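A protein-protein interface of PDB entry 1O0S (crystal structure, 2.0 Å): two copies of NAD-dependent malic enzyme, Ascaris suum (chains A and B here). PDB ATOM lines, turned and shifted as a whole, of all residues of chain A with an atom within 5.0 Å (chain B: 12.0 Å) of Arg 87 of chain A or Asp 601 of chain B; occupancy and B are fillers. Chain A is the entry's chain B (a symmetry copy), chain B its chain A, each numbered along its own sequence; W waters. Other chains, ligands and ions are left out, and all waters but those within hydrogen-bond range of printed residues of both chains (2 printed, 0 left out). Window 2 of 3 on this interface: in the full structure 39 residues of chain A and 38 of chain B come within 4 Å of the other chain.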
ATOM      1  N   ILE A  83       5.638 -23.662 -27.885  1.00  0.00           N
ATOM      2  CA  ILE A  83       6.758 -23.022 -27.205  1.00  0.00           C
ATOM      3  C   ILE A  83       6.686 -23.247 -25.696  1.00  0.00           C
ATOM      4  O   ILE A  83       7.708 -23.391 -25.034  1.00  0.00           O
ATOM      5  CB  ILE A  83       6.813 -21.519 -27.504  1.00  0.00           C
ATOM      6  CG1 ILE A  83       7.407 -21.303 -28.892  1.00  0.00           C
ATOM      7  CG2 ILE A  83       7.704 -20.809 -26.484  1.00  0.00           C
ATOM      8  CD1 ILE A  83       8.830 -21.839 -29.040  1.00  0.00           C
ATOM      9  N   THR A  84       5.475 -23.297 -25.155  1.00  0.00           N
ATOM     10  CA  THR A  84       5.328 -23.523 -23.729  1.00  0.00           C
ATOM     11  C   THR A  84       5.910 -24.877 -23.353  1.00  0.00           C
ATOM     12  O   THR A  84       6.762 -24.962 -22.469  1.00  0.00           O
ATOM     13  CB  THR A  84       3.851 -23.450 -23.299  1.00  0.00           C
ATOM     14  OG1 THR A  84       3.388 -22.104 -23.449  1.00  0.00           O
ATOM     15  CG2 THR A  84       3.689 -23.873 -21.839  1.00  0.00           C
ATOM     16  N   LYS A  85       5.462 -25.931 -24.033  1.00  0.00           N
ATOM     17  CA  LYS A  85       5.952 -27.266 -23.752  1.00  0.00           C
ATOM     18  C   LYS A  85       7.457 -27.379 -24.021  1.00  0.00           C
ATOM     19  O   LYS A  85       8.169 -28.109 -23.332  1.00  0.00           O
ATOM     20  CB  LYS A  85       5.173 -28.289 -24.587  1.00  0.00           C
ATOM     21  N   LEU A  86       7.934 -26.638 -25.014  1.00  0.00           N
ATOM     22  CA  LEU A  86       9.347 -26.640 -25.395  1.00  0.00           C
ATOM     23  C   LEU A  86      10.222 -26.100 -24.249  1.00  0.00           C
ATOM     24  O   LEU A  86      11.267 -26.665 -23.916  1.00  0.00           O
ATOM     25  CB  LEU A  86       9.526 -25.769 -26.641  1.00  0.00           C
ATOM     26  CG  LEU A  86      10.243 -26.287 -27.886  1.00  0.00           C
ATOM     27  CD1 LEU A  86       9.847 -27.707 -28.193  1.00  0.00           C
ATOM     28  CD2 LEU A  86       9.905 -25.370 -29.059  1.00  0.00           C
ATOM     29  N   ARG A  87       9.783 -24.997 -23.654  1.00  0.00           N
ATOM     30  CA  ARG A  87      10.521 -24.388 -22.560  1.00  0.00           C
ATOM     31  C   ARG A  87      10.357 -25.184 -21.273  1.00  0.00           C
ATOM     32  O   ARG A  87      11.166 -25.062 -20.354  1.00  0.00           O
ATOM     33  CB  ARG A  87      10.079 -22.933 -22.388  1.00  0.00           C
ATOM     34  CG  ARG A  87      10.569 -22.064 -23.549  1.00  0.00           C
ATOM     35  CD  ARG A  87      10.000 -20.658 -23.544  1.00  0.00           C
ATOM     36  NE  ARG A  87      10.482 -19.898 -24.692  1.00  0.00           N
ATOM     37  CZ  ARG A  87      10.095 -18.664 -25.004  1.00  0.00           C
ATOM     38  NH1 ARG A  87       9.205 -18.032 -24.256  1.00  0.00           N
ATOM     39  NH2 ARG A  87      10.605 -18.063 -26.069  1.00  0.00           N
ATOM     40  N   GLU A  88       9.329 -26.026 -21.219  1.00  0.00           N
ATOM     41  CA  GLU A  88       9.099 -26.851 -20.036  1.00  0.00           C
ATOM     42  C   GLU A  88       9.861 -28.174 -20.098  1.00  0.00           C
ATOM     43  O   GLU A  88       9.850 -28.939 -19.136  1.00  0.00           O
ATOM     44  CB  GLU A  88       7.605 -27.134 -19.851  1.00  0.00           C
ATOM     45  CG  GLU A  88       6.756 -25.883 -19.647  1.00  0.00           C
ATOM     46  CD  GLU A  88       5.329 -26.197 -19.218  1.00  0.00           C
ATOM     47  OE1 GLU A  88       4.754 -27.184 -19.728  1.00  0.00           O
ATOM     48  OE2 GLU A  88       4.780 -25.446 -18.380  1.00  0.00           O
ATOM     49  N   GLN A  89      10.516 -28.448 -21.226  1.00  0.00           N
ATOM     50  CA  GLN A  89      11.278 -29.684 -21.378  1.00  0.00           C
ATOM     51  C   GLN A  89      12.509 -29.650 -20.465  1.00  0.00           C
ATOM     52  O   GLN A  89      13.097 -28.599 -20.246  1.00  0.00           O
ATOM     53  CB  GLN A  89      11.716 -29.875 -22.837  1.00  0.00           C
ATOM     54  CG  GLN A  89      10.564 -30.025 -23.835  1.00  0.00           C
ATOM     55  CD  GLN A  89       9.859 -31.375 -23.747  1.00  0.00           C
ATOM     56  OE1 GLN A  89      10.126 -32.172 -22.857  1.00  0.00           O
ATOM     57  NE2 GLN A  89       8.949 -31.627 -24.683  1.00  0.00           N
ATOM     58  N   ARG A  95      13.926 -31.371 -26.119  1.00  0.00           N
ATOM     59  CA  ARG A  95      13.320 -30.396 -27.024  1.00  0.00           C
ATOM     60  C   ARG A  95      13.492 -30.893 -28.455  1.00  0.00           C
ATOM     61  O   ARG A  95      12.634 -30.660 -29.311  1.00  0.00           O
ATOM     62  CB  ARG A  95      13.954 -29.008 -26.850  1.00  0.00           C
ATOM     63  CG  ARG A  95      13.346 -28.201 -25.686  1.00  0.00           C
ATOM     64  CD  ARG A  95      13.978 -26.808 -25.520  1.00  0.00           C
ATOM     65  NE  ARG A  95      15.156 -26.838 -24.658  1.00  0.00           N
ATOM     66  CZ  ARG A  95      15.117 -26.957 -23.333  1.00  0.00           C
ATOM     67  NH1 ARG A  95      13.950 -27.048 -22.704  1.00  0.00           N
ATOM     68  NH2 ARG A  95      16.246 -27.016 -22.639  1.00  0.00           N
ATOM     69  N   HIS A 117      11.495 -18.354 -33.543  1.00  0.00           N
ATOM     70  CA  HIS A 117      12.464 -18.437 -32.455  1.00  0.00           C
ATOM     71  C   HIS A 117      13.760 -19.058 -32.983  1.00  0.00           C
ATOM     72  O   HIS A 117      14.256 -20.054 -32.446  1.00  0.00           O
ATOM     73  CB  HIS A 117      11.866 -19.308 -31.340  1.00  0.00           C
ATOM     74  CG  HIS A 117      10.517 -18.845 -30.867  1.00  0.00           C
ATOM     75  ND1 HIS A 117      10.356 -17.810 -29.969  1.00  0.00           N
ATOM     76  CD2 HIS A 117       9.271 -19.248 -31.206  1.00  0.00           C
ATOM     77  CE1 HIS A 117       9.064 -17.593 -29.778  1.00  0.00           C
ATOM     78  NE2 HIS A 117       8.384 -18.451 -30.516  1.00  0.00           N
ATOM     79  N   GLU A 120      16.821 -19.380 -30.661  1.00  0.00           N
ATOM     80  CA  GLU A 120      16.532 -20.340 -29.602  1.00  0.00           C
ATOM     81  C   GLU A 120      16.480 -21.789 -30.094  1.00  0.00           C
ATOM     82  O   GLU A 120      16.989 -22.705 -29.432  1.00  0.00           O
ATOM     83  CB  GLU A 120      15.183 -19.964 -28.957  1.00  0.00           C
ATOM     84  CG  GLU A 120      14.916 -20.537 -27.575  1.00  0.00           C
ATOM     85  CD  GLU A 120      13.500 -20.242 -27.073  1.00  0.00           C
ATOM     86  OE1 GLU A 120      12.968 -19.151 -27.359  1.00  0.00           O
ATOM     87  OE2 GLU A 120      12.923 -21.102 -26.378  1.00  0.00           O
ATOM     88  N   PHE B 593      -7.335 -18.637 -28.195  1.00  0.00           N
ATOM     89  CA  PHE B 593      -7.343 -19.026 -26.791  1.00  0.00           C
ATOM     90  C   PHE B 593      -8.710 -18.772 -26.167  1.00  0.00           C
ATOM     91  O   PHE B 593      -9.324 -17.720 -26.384  1.00  0.00           O
ATOM     92  CB  PHE B 593      -6.295 -18.247 -25.990  1.00  0.00           C
ATOM     93  CG  PHE B 593      -4.897 -18.751 -26.163  1.00  0.00           C
ATOM     94  CD1 PHE B 593      -3.992 -18.070 -26.967  1.00  0.00           C
ATOM     95  CD2 PHE B 593      -4.487 -19.921 -25.532  1.00  0.00           C
ATOM     96  CE1 PHE B 593      -2.694 -18.548 -27.142  1.00  0.00           C
ATOM     97  CE2 PHE B 593      -3.193 -20.409 -25.701  1.00  0.00           C
ATOM     98  CZ  PHE B 593      -2.296 -19.720 -26.508  1.00  0.00           C
ATOM     99  N   VAL B 597      -3.864 -15.148 -22.364  1.00  0.00           N
ATOM    100  CA  VAL B 597      -2.555 -15.347 -21.776  1.00  0.00           C
ATOM    101  C   VAL B 597      -1.657 -14.282 -22.379  1.00  0.00           C
ATOM    102  O   VAL B 597      -2.008 -13.675 -23.387  1.00  0.00           O
ATOM    103  CB  VAL B 597      -1.984 -16.743 -22.117  1.00  0.00           C
ATOM    104  CG1 VAL B 597      -2.740 -17.816 -21.350  1.00  0.00           C
ATOM    105  CG2 VAL B 597      -2.088 -16.998 -23.612  1.00  0.00           C
ATOM    106  N   VAL B 598      -0.509 -14.045 -21.753  1.00  0.00           N
ATOM    107  CA  VAL B 598       0.442 -13.069 -22.267  1.00  0.00           C
ATOM    108  C   VAL B 598       1.304 -13.777 -23.318  1.00  0.00           C
ATOM    109  O   VAL B 598       1.808 -14.878 -23.084  1.00  0.00           O
ATOM    110  CB  VAL B 598       1.331 -12.527 -21.132  1.00  0.00           C
ATOM    111  CG1 VAL B 598       2.420 -11.609 -21.695  1.00  0.00           C
ATOM    112  CG2 VAL B 598       0.470 -11.768 -20.134  1.00  0.00           C
ATOM    113  N   ARG B 599       1.466 -13.157 -24.480  1.00  0.00           N
ATOM    114  CA  ARG B 599       2.260 -13.767 -25.545  1.00  0.00           C
ATOM    115  C   ARG B 599       3.721 -13.952 -25.127  1.00  0.00           C
ATOM    116  O   ARG B 599       4.290 -13.104 -24.443  1.00  0.00           O
ATOM    117  CB  ARG B 599       2.186 -12.914 -26.821  1.00  0.00           C
ATOM    118  CG  ARG B 599       2.863 -13.562 -28.030  1.00  0.00           C
ATOM    119  CD  ARG B 599       2.681 -12.765 -29.318  1.00  0.00           C
ATOM    120  NE  ARG B 599       3.237 -13.474 -30.472  1.00  0.00           N
ATOM    121  CZ  ARG B 599       3.140 -13.058 -31.734  1.00  0.00           C
ATOM    122  NH1 ARG B 599       2.503 -11.928 -32.015  1.00  0.00           N
ATOM    123  NH2 ARG B 599       3.676 -13.773 -32.718  1.00  0.00           N
ATOM    124  N   HIS B 600       4.318 -15.072 -25.533  1.00  0.00           N
ATOM    125  CA  HIS B 600       5.718 -15.355 -25.220  1.00  0.00           C
ATOM    126  C   HIS B 600       6.609 -14.320 -25.896  1.00  0.00           C
ATOM    127  O   HIS B 600       6.153 -13.550 -26.744  1.00  0.00           O
ATOM    128  CB  HIS B 600       6.141 -16.730 -25.749  1.00  0.00           C
ATOM    129  CG  HIS B 600       5.438 -17.883 -25.108  1.00  0.00           C
ATOM    130  ND1 HIS B 600       5.357 -18.045 -23.743  1.00  0.00           N
ATOM    131  CD2 HIS B 600       4.823 -18.963 -25.651  1.00  0.00           C
ATOM    132  CE1 HIS B 600       4.722 -19.172 -23.470  1.00  0.00           C
ATOM    133  NE2 HIS B 600       4.389 -19.748 -24.612  1.00  0.00           N
ATOM    134  N   ASP B 601       7.883 -14.320 -25.517  1.00  0.00           N
ATOM    135  CA  ASP B 601       8.879 -13.423 -26.099  1.00  0.00           C
ATOM    136  C   ASP B 601       9.884 -14.335 -26.801  1.00  0.00           C
ATOM    137  O   ASP B 601       9.953 -15.519 -26.478  1.00  0.00           O
ATOM    138  CB  ASP B 601       9.571 -12.606 -25.005  1.00  0.00           C
ATOM    139  CG  ASP B 601       8.673 -11.519 -24.425  1.00  0.00           C
ATOM    140  OD1 ASP B 601       7.574 -11.843 -23.927  1.00  0.00           O
ATOM    141  OD2 ASP B 601       9.071 -10.336 -24.466  1.00  0.00           O
ATOM    142  N   SER B 602      10.655 -13.805 -27.750  1.00  0.00           N
ATOM    143  CA  SER B 602      11.635 -14.625 -28.478  1.00  0.00           C
ATOM    144  C   SER B 602      13.123 -14.287 -28.191  1.00  0.00           C
ATOM    145  O   SER B 602      13.526 -14.210 -27.036  1.00  0.00           O
ATOM    146  CB  SER B 602      11.360 -14.540 -29.990  1.00  0.00           C
ATOM    147  OG  SER B 602      11.440 -13.208 -30.471  1.00  0.00           O
ATOM    148  N   MET B 603      13.943 -14.067 -29.225  1.00  0.00           N
ATOM    149  CA  MET B 603      15.430 -13.762 -29.106  1.00  0.00           C
ATOM    150  C   MET B 603      16.298 -12.696 -28.310  1.00  0.00           C
ATOM    151  O   MET B 603      15.420 -11.871 -27.354  1.00  0.00           O
ATOM    152  CB  MET B 603      15.921 -13.778 -30.586  1.00  0.00           C
ATOM    153  CG  MET B 603      16.004 -12.359 -31.174  1.00  0.00           C
ATOM    154  SD  MET B 603      14.415 -11.525 -31.458  1.00  0.00           S
ATOM    155  CE  MET B 603      14.481 -10.163 -30.274  1.00  0.00           C
HETATM  156  O   HOH W   1       7.833 -18.853 -21.726  1.00  0.00           O
HETATM  157  O   HOH W   2      14.891 -17.146 -30.547  1.00  0.00           O
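A ring nitrogen (NE2) of His 600 of chain B lies within hydrogen-bond range of the side-chain hydroxyl (OG1) of Thr 84 of chain A (2.8 Å). The guanidinium group of Arg 87 of chain A lies within hydrogen-bond range of the backbone carbonyl oxygen of Asp 601 of chain B, at 2.7 Å.
OG of Ser 602 of chain B lies within hydrogen-bond range of SD of Met 603 of chain B (3.6 Å). NH2 of Arg 87 of chain A lies within salt-bridge range of OE1 of Glu 120 of chain A (2.9 Å).
Among the printed residues, pairs that only touch across the chains: His 117 of chain A with Ser 602 of chain B (3.4 Å), Ile 83 of chain A with His 600 of chain B (3.5 Å), Arg 87 of chain A with His 600 of chain B (3.6 Å) and His 117 of chain A with Asp 601 of chain B (3.998 Å).
Of chain B, only His 600 (3.6 Å) and Asp 601 (2.7 Å) come within 4 Å of Arg 87 of chain A. Of the printed residues of chain A, Asp 601 of chain B touches Arg 87 and His 117. Ile 83 of chain A touches just one residue of chain B: His 600. Of the printed residues of chain B, Thr 84 of chain A touches His 600. No residue of chain B comes within 4 Å of Lys 85 of chain A. No residue of chain B comes within 4 Å of Leu 86 of chain A. No residue of chain B comes within 4 Å of Glu 88 of chain A. No residue of chain B comes within 4 Å of Gln 89 of chain A. Printed residues of chain B within 4 Å of His 117 of chain A: Asp 601 and Ser 602. Printed residues of chain A within 4 Å of Ser 602 of chain B: His 117 (3.4 Å). Of the printed residues of chain A, His 600 of chain B touches Ile 83, Thr 84 and Arg 87. Arg 599 of chain B touches none of the printed residues of chain A. The nearest residue of chain B that does not touch Arg 87 of chain A is Ser 602 of chain B (4.3 Å).
Printed residues of chain A that touch a printed residue of chain B: Ile 83, Thr 84, Arg 87 and His 117. Hydrophobic or aromatic side chains of chain A that line the printed part of chain B: Ile 83 and His 117. Along chain A the printed residues that touch a printed residue of chain B span positions 83 to 117. Printed residues of chain B that touch a printed residue of chain A: His 600, Asp 601 and Ser 602. Among the printed residues, 6 pairs touch across the chains.
No position is printed for both chains.
Water W2 lies within hydrogen-bond range of the backbone NH of Glu 120 of chain A and the backbone NH of Met 603 of chain B. Water W1 lies within hydrogen-bond range of the guanidinium group (NH1) of Arg 87 of chain A (3.0 Å) and a ring nitrogen (ND1) of His 600 of chain B (3.3 Å).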
